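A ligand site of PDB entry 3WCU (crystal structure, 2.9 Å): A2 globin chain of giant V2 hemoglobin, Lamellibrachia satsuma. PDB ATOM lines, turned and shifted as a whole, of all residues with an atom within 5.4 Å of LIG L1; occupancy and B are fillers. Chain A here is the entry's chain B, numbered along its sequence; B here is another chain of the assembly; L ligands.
Merely in contact with LIG L1: Met 46, Phe 47, Val 50, His 63, Arg 66, Gly 70, Leu 71, Leu 91, Gln 94 of chain A, Arg 98 of chain A, Val 100, Gln 104, Tyr 105 and Ile 141. Hydrophobic or aromatic side chains within 4 Å of LIG L1: Met 46, Phe 47, Val 50, His 63, Leu 71, Leu 91, His 95, Val 100, Tyr 105, Ile 141 and His 94 of chain B.
A ring nitrogen (ND1) of His 95 is in hydrogen-bond range of the backbone carbonyl oxygen (O) of Leu 91 (3.2 Å). The guanidinium group (NH2) of Arg 49 lies close to a ring nitrogen (ND1) of His 94 of chain B (3.4 Å). NH2 of Arg 66 sits at hydrogen-bond distance from ND1 of His 94 of chain B (3.4 Å). The side-chain amide oxygen (OE1) of Gln 104 sits close to the side-chain sulfur (SD) of Met 46, at 3.5 Å. NE of Arg 98 of chain A sits at hydrogen-bond distance from O of Gln 94 of chain A (2.7 Å). The guanidinium group (NH1) of Arg 66 lies close to a ring nitrogen (ND1) of His 63, 3.3 Å away.
A ring nitrogen (NE2) of His 95 is bound to an iron atom (FE1) of LIG L1. The guanidinium group (NE) of Arg 49 is in salt-bridge range of an oxygen (O4) of LIG L1 (2.8 Å). An oxygen (O2) of LIG L1 is in hydrogen-bond range of a ring nitrogen (NE2) of His 94 of chain B, 2.9 Å away. The side-chain amide nitrogen (NE2) of Gln 98 of chain B is in hydrogen-bond range of an oxygen (O2) of LIG L1. The side-chain amide nitrogen of Gln 94 of chain A sits at hydrogen-bond distance from an oxygen (O1) of LG2 L2 (3.4 Å).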
ATOM      1  N   ALA A  43      13.653  38.329   4.893  1.00  0.00           N
ATOM      2  CA  ALA A  43      14.069  37.422   3.840  1.00  0.00           C
ATOM      3  C   ALA A  43      14.824  38.022   2.666  1.00  0.00           C
ATOM      4  O   ALA A  43      15.703  37.370   2.104  1.00  0.00           O
ATOM      5  CB  ALA A  43      12.855  36.655   3.318  1.00  0.00           C
ATOM      6  N   MET A  46      18.579  37.547   1.508  1.00  0.00           N
ATOM      7  CA  MET A  46      19.102  36.336   0.882  1.00  0.00           C
ATOM      8  C   MET A  46      19.155  36.484  -0.636  1.00  0.00           C
ATOM      9  O   MET A  46      19.918  35.788  -1.308  1.00  0.00           O
ATOM     10  CB  MET A  46      18.224  35.147   1.248  1.00  0.00           C
ATOM     11  CG  MET A  46      18.067  34.988   2.743  1.00  0.00           C
ATOM     12  SD  MET A  46      17.098  33.566   3.193  1.00  0.00           S
ATOM     13  CE  MET A  46      18.312  32.260   2.975  1.00  0.00           C
ATOM     14  N   PHE A  47      18.350  37.395  -1.147  1.00  0.00           N
ATOM     15  CA  PHE A  47      18.289  37.648  -2.582  1.00  0.00           C
ATOM     16  C   PHE A  47      19.053  38.913  -2.890  1.00  0.00           C
ATOM     17  O   PHE A  47      18.642  39.726  -3.723  1.00  0.00           O
ATOM     18  CB  PHE A  47      16.821  37.767  -3.008  1.00  0.00           C
ATOM     19  CG  PHE A  47      15.965  36.653  -2.488  1.00  0.00           C
ATOM     20  CD1 PHE A  47      16.100  35.361  -2.991  1.00  0.00           C
ATOM     21  CD2 PHE A  47      15.070  36.886  -1.436  1.00  0.00           C
ATOM     22  CE1 PHE A  47      15.355  34.307  -2.462  1.00  0.00           C
ATOM     23  CE2 PHE A  47      14.317  35.833  -0.891  1.00  0.00           C
ATOM     24  CZ  PHE A  47      14.460  34.540  -1.410  1.00  0.00           C
ATOM     25  N   ARG A  49      21.998  39.078  -4.262  1.00  0.00           N
ATOM     26  CA  ARG A  49      22.629  38.966  -5.583  1.00  0.00           C
ATOM     27  C   ARG A  49      21.652  39.179  -6.766  1.00  0.00           C
ATOM     28  O   ARG A  49      22.074  39.430  -7.888  1.00  0.00           O
ATOM     29  CB  ARG A  49      23.313  37.623  -5.733  1.00  0.00           C
ATOM     30  CG  ARG A  49      24.192  37.506  -6.976  1.00  0.00           C
ATOM     31  CD  ARG A  49      24.629  36.075  -7.198  1.00  0.00           C
ATOM     32  NE  ARG A  49      23.537  35.274  -7.745  1.00  0.00           N
ATOM     33  CZ  ARG A  49      23.132  35.349  -9.008  1.00  0.00           C
ATOM     34  NH1 ARG A  49      23.738  36.184  -9.841  1.00  0.00           N
ATOM     35  NH2 ARG A  49      22.126  34.602  -9.428  1.00  0.00           N
ATOM     36  N   VAL A  50      20.348  39.073  -6.481  1.00  0.00           N
ATOM     37  CA  VAL A  50      19.284  39.258  -7.455  1.00  0.00           C
ATOM     38  C   VAL A  50      18.371  40.440  -7.048  1.00  0.00           C
ATOM     39  O   VAL A  50      17.156  40.390  -7.145  1.00  0.00           O
ATOM     40  CB  VAL A  50      18.445  37.974  -7.532  1.00  0.00           C
ATOM     41  CG1 VAL A  50      19.137  36.952  -8.368  1.00  0.00           C
ATOM     42  CG2 VAL A  50      18.203  37.462  -6.137  1.00  0.00           C
ATOM     43  N   HIS A  63      14.919  36.422 -11.432  1.00  0.00           N
ATOM     44  CA  HIS A  63      15.104  35.503 -10.316  1.00  0.00           C
ATOM     45  C   HIS A  63      13.792  34.765 -10.032  1.00  0.00           C
ATOM     46  O   HIS A  63      13.752  33.525 -10.064  1.00  0.00           O
ATOM     47  CB  HIS A  63      15.536  36.250  -9.041  1.00  0.00           C
ATOM     48  CG  HIS A  63      15.404  35.435  -7.785  1.00  0.00           C
ATOM     49  ND1 HIS A  63      16.137  34.284  -7.570  1.00  0.00           N
ATOM     50  CD2 HIS A  63      14.561  35.548  -6.735  1.00  0.00           C
ATOM     51  CE1 HIS A  63      15.734  33.718  -6.444  1.00  0.00           C
ATOM     52  NE2 HIS A  63      14.776  34.464  -5.923  1.00  0.00           N
ATOM     53  N   ARG A  66      13.022  32.257 -12.251  1.00  0.00           N
ATOM     54  CA  ARG A  66      13.817  31.057 -11.948  1.00  0.00           C
ATOM     55  C   ARG A  66      13.211  30.228 -10.816  1.00  0.00           C
ATOM     56  O   ARG A  66      13.164  28.989 -10.890  1.00  0.00           O
ATOM     57  CB  ARG A  66      15.254  31.460 -11.598  1.00  0.00           C
ATOM     58  CG  ARG A  66      16.317  31.018 -12.620  1.00  0.00           C
ATOM     59  CD  ARG A  66      17.368  32.103 -12.780  1.00  0.00           C
ATOM     60  NE  ARG A  66      17.677  32.735 -11.499  1.00  0.00           N
ATOM     61  CZ  ARG A  66      17.961  34.027 -11.350  1.00  0.00           C
ATOM     62  NH1 ARG A  66      18.217  34.494 -10.130  1.00  0.00           N
ATOM     63  NH2 ARG A  66      17.990  34.831 -12.398  1.00  0.00           N
ATOM     64  N   VAL A  67      12.733  30.915  -9.776  1.00  0.00           N
ATOM     65  CA  VAL A  67      12.107  30.230  -8.646  1.00  0.00           C
ATOM     66  C   VAL A  67      10.809  29.535  -9.059  1.00  0.00           C
ATOM     67  O   VAL A  67      10.743  28.291  -9.065  1.00  0.00           O
ATOM     68  CB  VAL A  67      11.765  31.208  -7.493  1.00  0.00           C
ATOM     69  CG1 VAL A  67      10.951  30.500  -6.431  1.00  0.00           C
ATOM     70  CG2 VAL A  67      13.048  31.776  -6.884  1.00  0.00           C
ATOM     71  N   GLY A  70      10.952  26.733 -11.088  1.00  0.00           N
ATOM     72  CA  GLY A  70      11.294  25.493 -10.427  1.00  0.00           C
ATOM     73  C   GLY A  70      10.085  24.871  -9.757  1.00  0.00           C
ATOM     74  O   GLY A  70       9.854  23.651  -9.840  1.00  0.00           O
ATOM     75  N   LEU A  71       9.296  25.705  -9.084  1.00  0.00           N
ATOM     76  CA  LEU A  71       8.107  25.245  -8.392  1.00  0.00           C
ATOM     77  C   LEU A  71       7.292  24.444  -9.397  1.00  0.00           C
ATOM     78  O   LEU A  71       6.664  23.449  -9.045  1.00  0.00           O
ATOM     79  CB  LEU A  71       7.276  26.432  -7.870  1.00  0.00           C
ATOM     80  CG  LEU A  71       6.559  26.247  -6.519  1.00  0.00           C
ATOM     81  CD1 LEU A  71       5.674  27.469  -6.240  1.00  0.00           C
ATOM     82  CD2 LEU A  71       5.738  24.946  -6.504  1.00  0.00           C
ATOM     83  N   CYS A  74       8.519  20.827 -10.135  1.00  0.00           N
ATOM     84  CA  CYS A  74       8.055  19.977  -9.050  1.00  0.00           C
ATOM     85  C   CYS A  74       6.590  19.604  -9.140  1.00  0.00           C
ATOM     86  O   CYS A  74       6.251  18.410  -9.161  1.00  0.00           O
ATOM     87  CB  CYS A  74       8.344  20.653  -7.698  1.00  0.00           C
ATOM     88  SG  CYS A  74      10.101  20.752  -7.249  1.00  0.00           S
ATOM     89  N   LEU A  91      17.400  19.842  -5.862  1.00  0.00           N
ATOM     90  CA  LEU A  91      17.079  21.182  -5.378  1.00  0.00           C
ATOM     91  C   LEU A  91      17.562  21.376  -3.958  1.00  0.00           C
ATOM     92  O   LEU A  91      17.866  22.494  -3.543  1.00  0.00           O
ATOM     93  CB  LEU A  91      15.562  21.433  -5.399  1.00  0.00           C
ATOM     94  CG  LEU A  91      14.835  22.174  -6.529  1.00  0.00           C
ATOM     95  CD1 LEU A  91      13.438  22.504  -6.027  1.00  0.00           C
ATOM     96  CD2 LEU A  91      15.550  23.466  -6.912  1.00  0.00           C
ATOM     97  N   GLN A  94      20.973  22.496  -3.520  1.00  0.00           N
ATOM     98  CA  GLN A  94      21.129  23.861  -4.007  1.00  0.00           C
ATOM     99  C   GLN A  94      20.694  24.934  -3.003  1.00  0.00           C
ATOM    100  O   GLN A  94      21.064  26.090  -3.163  1.00  0.00           O
ATOM    101  CB  GLN A  94      20.349  24.067  -5.302  1.00  0.00           C
ATOM    102  CG  GLN A  94      21.165  23.922  -6.580  1.00  0.00           C
ATOM    103  CD  GLN A  94      20.333  24.184  -7.819  1.00  0.00           C
ATOM    104  OE1 GLN A  94      19.477  25.077  -7.830  1.00  0.00           O
ATOM    105  NE2 GLN A  94      20.565  23.409  -8.874  1.00  0.00           N
ATOM    106  N   HIS A  95      19.926  24.556  -1.992  1.00  0.00           N
ATOM    107  CA  HIS A  95      19.452  25.527  -0.994  1.00  0.00           C
ATOM    108  C   HIS A  95      20.046  25.325   0.406  1.00  0.00           C
ATOM    109  O   HIS A  95      19.615  25.957   1.381  1.00  0.00           O
ATOM    110  CB  HIS A  95      17.901  25.490  -0.923  1.00  0.00           C
ATOM    111  CG  HIS A  95      17.210  26.085  -2.106  1.00  0.00           C
ATOM    112  ND1 HIS A  95      17.355  25.605  -3.392  1.00  0.00           N
ATOM    113  CD2 HIS A  95      16.376  27.154  -2.210  1.00  0.00           C
ATOM    114  CE1 HIS A  95      16.651  26.342  -4.225  1.00  0.00           C
ATOM    115  NE2 HIS A  95      16.042  27.285  -3.544  1.00  0.00           N
ATOM    116  N   ARG A  98      22.644  28.044   1.152  1.00  0.00           N
ATOM    117  CA  ARG A  98      21.914  29.308   1.208  1.00  0.00           C
ATOM    118  C   ARG A  98      21.313  29.530   2.587  1.00  0.00           C
ATOM    119  O   ARG A  98      20.708  30.566   2.846  1.00  0.00           O
ATOM    120  CB  ARG A  98      20.806  29.320   0.144  1.00  0.00           C
ATOM    121  CG  ARG A  98      21.285  29.005  -1.275  1.00  0.00           C
ATOM    122  CD  ARG A  98      20.166  29.175  -2.300  1.00  0.00           C
ATOM    123  NE  ARG A  98      20.505  28.667  -3.629  1.00  0.00           N
ATOM    124  CZ  ARG A  98      21.503  29.120  -4.397  1.00  0.00           C
ATOM    125  NH1 ARG A  98      21.720  28.582  -5.590  1.00  0.00           N
ATOM    126  NH2 ARG A  98      22.276  30.104  -3.968  1.00  0.00           N
ATOM    127  N   VAL A 100      18.594  28.379   4.403  1.00  0.00           N
ATOM    128  CA  VAL A 100      17.190  28.761   4.441  1.00  0.00           C
ATOM    129  C   VAL A 100      16.458  28.073   5.585  1.00  0.00           C
ATOM    130  O   VAL A 100      16.486  26.847   5.711  1.00  0.00           O
ATOM    131  CB  VAL A 100      16.494  28.390   3.108  1.00  0.00           C
ATOM    132  CG1 VAL A 100      15.055  28.875   3.126  1.00  0.00           C
ATOM    133  CG2 VAL A 100      17.250  29.004   1.935  1.00  0.00           C
ATOM    134  N   GLN A 104      10.898  29.754   6.564  1.00  0.00           N
ATOM    135  CA  GLN A 104      10.824  30.526   5.341  1.00  0.00           C
ATOM    136  C   GLN A 104      10.210  29.719   4.200  1.00  0.00           C
ATOM    137  O   GLN A 104       9.511  30.264   3.341  1.00  0.00           O
ATOM    138  CB  GLN A 104      12.226  31.027   4.969  1.00  0.00           C
ATOM    139  CG  GLN A 104      12.787  31.968   6.022  1.00  0.00           C
ATOM    140  CD  GLN A 104      14.166  32.486   5.664  1.00  0.00           C
ATOM    141  OE1 GLN A 104      15.112  31.719   5.482  1.00  0.00           O
ATOM    142  NE2 GLN A 104      14.296  33.816   5.581  1.00  0.00           N
ATOM    143  N   TYR A 105      10.464  28.413   4.193  1.00  0.00           N
ATOM    144  CA  TYR A 105       9.895  27.544   3.172  1.00  0.00           C
ATOM    145  C   TYR A 105       8.399  27.466   3.417  1.00  0.00           C
ATOM    146  O   TYR A 105       7.685  26.775   2.696  1.00  0.00           O
ATOM    147  CB  TYR A 105      10.485  26.139   3.268  1.00  0.00           C
ATOM    148  CG  TYR A 105      11.883  25.973   2.695  1.00  0.00           C
ATOM    149  CD1 TYR A 105      12.082  25.729   1.346  1.00  0.00           C
ATOM    150  CD2 TYR A 105      13.005  26.052   3.525  1.00  0.00           C
ATOM    151  CE1 TYR A 105      13.363  25.561   0.827  1.00  0.00           C
ATOM    152  CE2 TYR A 105      14.292  25.883   3.015  1.00  0.00           C
ATOM    153  CZ  TYR A 105      14.462  25.635   1.659  1.00  0.00           C
ATOM    154  OH  TYR A 105      15.737  25.482   1.156  1.00  0.00           O
ATOM    155  N   VAL A 108       6.812  31.312   1.944  1.00  0.00           N
ATOM    156  CA  VAL A 108       6.775  31.328   0.493  1.00  0.00           C
ATOM    157  C   VAL A 108       5.628  30.411   0.084  1.00  0.00           C
ATOM    158  O   VAL A 108       4.917  30.695  -0.877  1.00  0.00           O
ATOM    159  CB  VAL A 108       8.132  30.818  -0.102  1.00  0.00           C
ATOM    160  CG1 VAL A 108       7.879  29.774  -1.198  1.00  0.00           C
ATOM    161  CG2 VAL A 108       8.921  31.981  -0.661  1.00  0.00           C
ATOM    162  N   ILE A 137       6.626  19.312  -1.337  1.00  0.00           N
ATOM    163  CA  ILE A 137       7.669  19.832  -2.208  1.00  0.00           C
ATOM    164  C   ILE A 137       8.769  20.539  -1.417  1.00  0.00           C
ATOM    165  O   ILE A 137       9.931  20.518  -1.813  1.00  0.00           O
ATOM    166  CB  ILE A 137       7.082  20.799  -3.276  1.00  0.00           C
ATOM    167  CG1 ILE A 137       6.305  19.988  -4.314  1.00  0.00           C
ATOM    168  CG2 ILE A 137       8.183  21.589  -3.967  1.00  0.00           C
ATOM    169  CD1 ILE A 137       5.798  20.813  -5.460  1.00  0.00           C
ATOM    170  N   THR A 138       8.397  21.157  -0.292  1.00  0.00           N
ATOM    171  CA  THR A 138       9.373  21.849   0.544  1.00  0.00           C
ATOM    172  C   THR A 138      10.140  20.891   1.466  1.00  0.00           C
ATOM    173  O   THR A 138      11.334  21.064   1.720  1.00  0.00           O
ATOM    174  CB  THR A 138       8.693  22.983   1.381  1.00  0.00           C
ATOM    175  OG1 THR A 138       7.506  22.494   2.024  1.00  0.00           O
ATOM    176  CG2 THR A 138       8.326  24.155   0.488  1.00  0.00           C
ATOM    177  N   ILE A 141      13.149  19.800  -0.425  1.00  0.00           N
ATOM    178  CA  ILE A 141      14.195  20.772  -0.716  1.00  0.00           C
ATOM    179  C   ILE A 141      14.989  20.920   0.570  1.00  0.00           C
ATOM    180  O   ILE A 141      16.182  21.214   0.556  1.00  0.00           O
ATOM    181  CB  ILE A 141      13.576  22.132  -1.097  1.00  0.00           C
ATOM    182  CG1 ILE A 141      12.561  21.922  -2.216  1.00  0.00           C
ATOM    183  CG2 ILE A 141      14.678  23.099  -1.547  1.00  0.00           C
ATOM    184  CD1 ILE A 141      11.738  23.139  -2.513  1.00  0.00           C
ATOM    185  N   HIS B  94      22.174  35.034 -17.212  1.00  0.00           N
ATOM    186  CA  HIS B  94      22.412  34.266 -16.002  1.00  0.00           C
ATOM    187  C   HIS B  94      22.546  32.824 -16.467  1.00  0.00           C
ATOM    188  O   HIS B  94      23.254  32.023 -15.859  1.00  0.00           O
ATOM    189  CB  HIS B  94      21.229  34.408 -15.022  1.00  0.00           C
ATOM    190  CG  HIS B  94      21.231  33.402 -13.912  1.00  0.00           C
ATOM    191  ND1 HIS B  94      21.162  33.760 -12.584  1.00  0.00           N
ATOM    192  CD2 HIS B  94      21.224  32.045 -13.924  1.00  0.00           C
ATOM    193  CE1 HIS B  94      21.097  32.677 -11.832  1.00  0.00           C
ATOM    194  NE2 HIS B  94      21.133  31.616 -12.621  1.00  0.00           N
ATOM    195  N   GLN B  98      26.106  30.483 -16.503  1.00  0.00           N
ATOM    196  CA  GLN B  98      25.805  29.155 -15.978  1.00  0.00           C
ATOM    197  C   GLN B  98      26.116  27.995 -16.953  1.00  0.00           C
ATOM    198  O   GLN B  98      26.288  26.852 -16.534  1.00  0.00           O
ATOM    199  CB  GLN B  98      24.324  29.102 -15.567  1.00  0.00           C
ATOM    200  CG  GLN B  98      23.931  27.882 -14.764  1.00  0.00           C
ATOM    201  CD  GLN B  98      22.428  27.641 -14.802  1.00  0.00           C
ATOM    202  OE1 GLN B  98      21.870  27.219 -15.813  1.00  0.00           O
ATOM    203  NE2 GLN B  98      21.766  27.927 -13.682  1.00  0.00           N
HETATM  204  C1  LIG L   1      17.703  30.120  -5.978  1.00  0.00           C
HETATM  205  C2  LIG L   1      14.102  27.107  -6.622  1.00  0.00           C
HETATM  206  C3  LIG L   1      12.386  28.154  -2.210  1.00  0.00           C
HETATM  207  C4  LIG L   1      16.061  31.188  -1.641  1.00  0.00           C
HETATM  208  C5  LIG L   1      16.879  29.227  -6.569  1.00  0.00           C
HETATM  209  C6  LIG L   1      17.081  28.769  -7.875  1.00  0.00           C
HETATM  210  C7  LIG L   1      16.071  27.887  -8.094  1.00  0.00           C
HETATM  211  C8  LIG L   1      15.221  27.823  -6.867  1.00  0.00           C
HETATM  212  C9  LIG L   1      15.778  27.069  -9.372  1.00  0.00           C
HETATM  213  C10 LIG L   1      18.230  29.235  -8.809  1.00  0.00           C
HETATM  214  C11 LIG L   1      18.988  28.212  -9.602  1.00  0.00           C
HETATM  215  C12 LIG L   1      20.094  28.810 -10.491  1.00  0.00           C
HETATM  216  O1  LIG L   1      21.295  28.762 -10.116  1.00  0.00           O
HETATM  217  O2  LIG L   1      19.784  29.322 -11.538  1.00  0.00           O
HETATM  218  C13 LIG L   1      13.280  27.090  -5.455  1.00  0.00           C
HETATM  219  C14 LIG L   1      12.089  26.275  -5.302  1.00  0.00           C
HETATM  220  C15 LIG L   1      11.592  26.601  -3.987  1.00  0.00           C
HETATM  221  C16 LIG L   1      12.505  27.563  -3.466  1.00  0.00           C
HETATM  222  C17 LIG L   1      11.519  25.322  -6.282  1.00  0.00           C
HETATM  223  C18 LIG L   1      10.384  26.014  -3.419  1.00  0.00           C
HETATM  224  C19 LIG L   1       9.177  26.496  -3.556  1.00  0.00           C
HETATM  225  C20 LIG L   1      13.255  29.092  -1.677  1.00  0.00           C
HETATM  226  C21 LIG L   1      13.062  29.706  -0.355  1.00  0.00           C
HETATM  227  C22 LIG L   1      14.122  30.604  -0.152  1.00  0.00           C
HETATM  228  C23 LIG L   1      14.934  30.480  -1.426  1.00  0.00           C
HETATM  229  C24 LIG L   1      11.916  29.417   0.623  1.00  0.00           C
HETATM  230  C25 LIG L   1      14.341  31.402   0.914  1.00  0.00           C
HETATM  231  C26 LIG L   1      13.946  32.544   1.348  1.00  0.00           C
HETATM  232  C27 LIG L   1      16.856  31.144  -2.774  1.00  0.00           C
HETATM  233  C28 LIG L   1      18.104  31.966  -2.970  1.00  0.00           C
HETATM  234  C29 LIG L   1      18.546  31.625  -4.221  1.00  0.00           C
HETATM  235  C30 LIG L   1      17.592  30.653  -4.754  1.00  0.00           C
HETATM  236  C31 LIG L   1      18.700  32.932  -1.947  1.00  0.00           C
HETATM  237  C32 LIG L   1      19.769  32.133  -4.963  1.00  0.00           C
HETATM  238  C33 LIG L   1      19.471  33.212  -5.947  1.00  0.00           C
HETATM  239  C34 LIG L   1      20.676  33.643  -6.662  1.00  0.00           C
HETATM  240  O3  LIG L   1      21.278  32.800  -7.402  1.00  0.00           O
HETATM  241  O4  LIG L   1      21.084  34.801  -6.544  1.00  0.00           O
HETATM  242  N1  LIG L   1      15.745  28.675  -5.937  1.00  0.00           N
HETATM  243  N2  LIG L   1      13.553  27.847  -4.388  1.00  0.00           N
HETATM  244  N3  LIG L   1      14.400  29.600  -2.283  1.00  0.00           N
HETATM  245  N4  LIG L   1      16.607  30.384  -3.855  1.00  0.00           N
HETATM  246 FE1  LIG L   1      15.079  29.108  -4.093  1.00  0.00          FE
HETATM  247  C1  LG2 L   2      21.978  22.386 -17.512  1.00  0.00           C
HETATM  248  C2  LG2 L   2      18.708  24.918 -19.827  1.00  0.00           C
HETATM  249  C3  LG2 L   2      20.908  24.040 -24.067  1.00  0.00           C
HETATM  250  C4  LG2 L   2      24.249  21.536 -21.674  1.00  0.00           C
HETATM  251  C5  LG2 L   2      20.880  23.149 -17.751  1.00  0.00           C
HETATM  252  C6  LG2 L   2      19.978  23.553 -16.742  1.00  0.00           C
HETATM  253  C7  LG2 L   2      19.046  24.285 -17.399  1.00  0.00           C
HETATM  254  C8  LG2 L   2      19.383  24.333 -18.831  1.00  0.00           C
HETATM  255  C9  LG2 L   2      17.805  24.975 -16.790  1.00  0.00           C
HETATM  256  C10 LG2 L   2      20.029  23.201 -15.249  1.00  0.00           C
HETATM  257  C11 LG2 L   2      20.158  24.344 -14.273  1.00  0.00           C
HETATM  258  C12 LG2 L   2      20.183  23.910 -12.782  1.00  0.00           C
HETATM  259  O1  LG2 L   2      19.669  24.672 -11.902  1.00  0.00           O
HETATM  260  O2  LG2 L   2      20.661  22.835 -12.499  1.00  0.00           O
HETATM  261  C13 LG2 L   2      18.990  24.922 -21.219  1.00  0.00           C
HETATM  262  C14 LG2 L   2      18.169  25.572 -22.210  1.00  0.00           C
HETATM  263  C15 LG2 L   2      18.831  25.301 -23.477  1.00  0.00           C
HETATM  264  C16 LG2 L   2      19.976  24.526 -23.139  1.00  0.00           C
HETATM  265  C17 LG2 L   2      16.935  26.326 -21.958  1.00  0.00           C
HETATM  266  C18 LG2 L   2      18.332  25.748 -24.755  1.00  0.00           C
HETATM  267  C19 LG2 L   2      18.661  26.882 -25.354  1.00  0.00           C
HETATM  268  C20 LG2 L   2      22.046  23.273 -23.758  1.00  0.00           C
HETATM  269  C21 LG2 L   2      22.975  22.781 -24.789  1.00  0.00           C
HETATM  270  C22 LG2 L   2      23.973  22.056 -24.133  1.00  0.00           C
HETATM  271  C23 LG2 L   2      23.563  22.137 -22.664  1.00  0.00           C
HETATM  272  C24 LG2 L   2      22.879  23.024 -26.284  1.00  0.00           C
HETATM  273  C25 LG2 L   2      25.035  21.428 -24.694  1.00  0.00           C
HETATM  274  C26 LG2 L   2      25.481  20.252 -24.918  1.00  0.00           C
HETATM  275  C27 LG2 L   2      23.915  21.553 -20.321  1.00  0.00           C
HETATM  276  C28 LG2 L   2      24.716  20.840 -19.254  1.00  0.00           C
HETATM  277  C29 LG2 L   2      24.038  21.092 -18.082  1.00  0.00           C
HETATM  278  C30 LG2 L   2      22.889  21.931 -18.425  1.00  0.00           C
HETATM  279  C31 LG2 L   2      25.975  20.033 -19.524  1.00  0.00           C
HETATM  280  C32 LG2 L   2      24.372  20.619 -16.689  1.00  0.00           C
HETATM  281  C33 LG2 L   2      23.586  19.363 -16.379  1.00  0.00           C
HETATM  282  C34 LG2 L   2      23.809  18.795 -15.033  1.00  0.00           C
HETATM  283  O3  LG2 L   2      24.280  17.601 -14.925  1.00  0.00           O
HETATM  284  O4  LG2 L   2      23.515  19.484 -14.028  1.00  0.00           O
HETATM  285  N1  LG2 L   2      20.525  23.624 -19.039  1.00  0.00           N
HETATM  286  N2  LG2 L   2      20.071  24.298 -21.734  1.00  0.00           N
HETATM  287  N3  LG2 L   2      22.438  22.852 -22.499  1.00  0.00           N
HETATM  288  N4  LG2 L   2      22.860  22.180 -19.775  1.00  0.00           N
HETATM  289 FE1  LG2 L   2      21.489  23.265 -20.760  1.00  0.00          FE
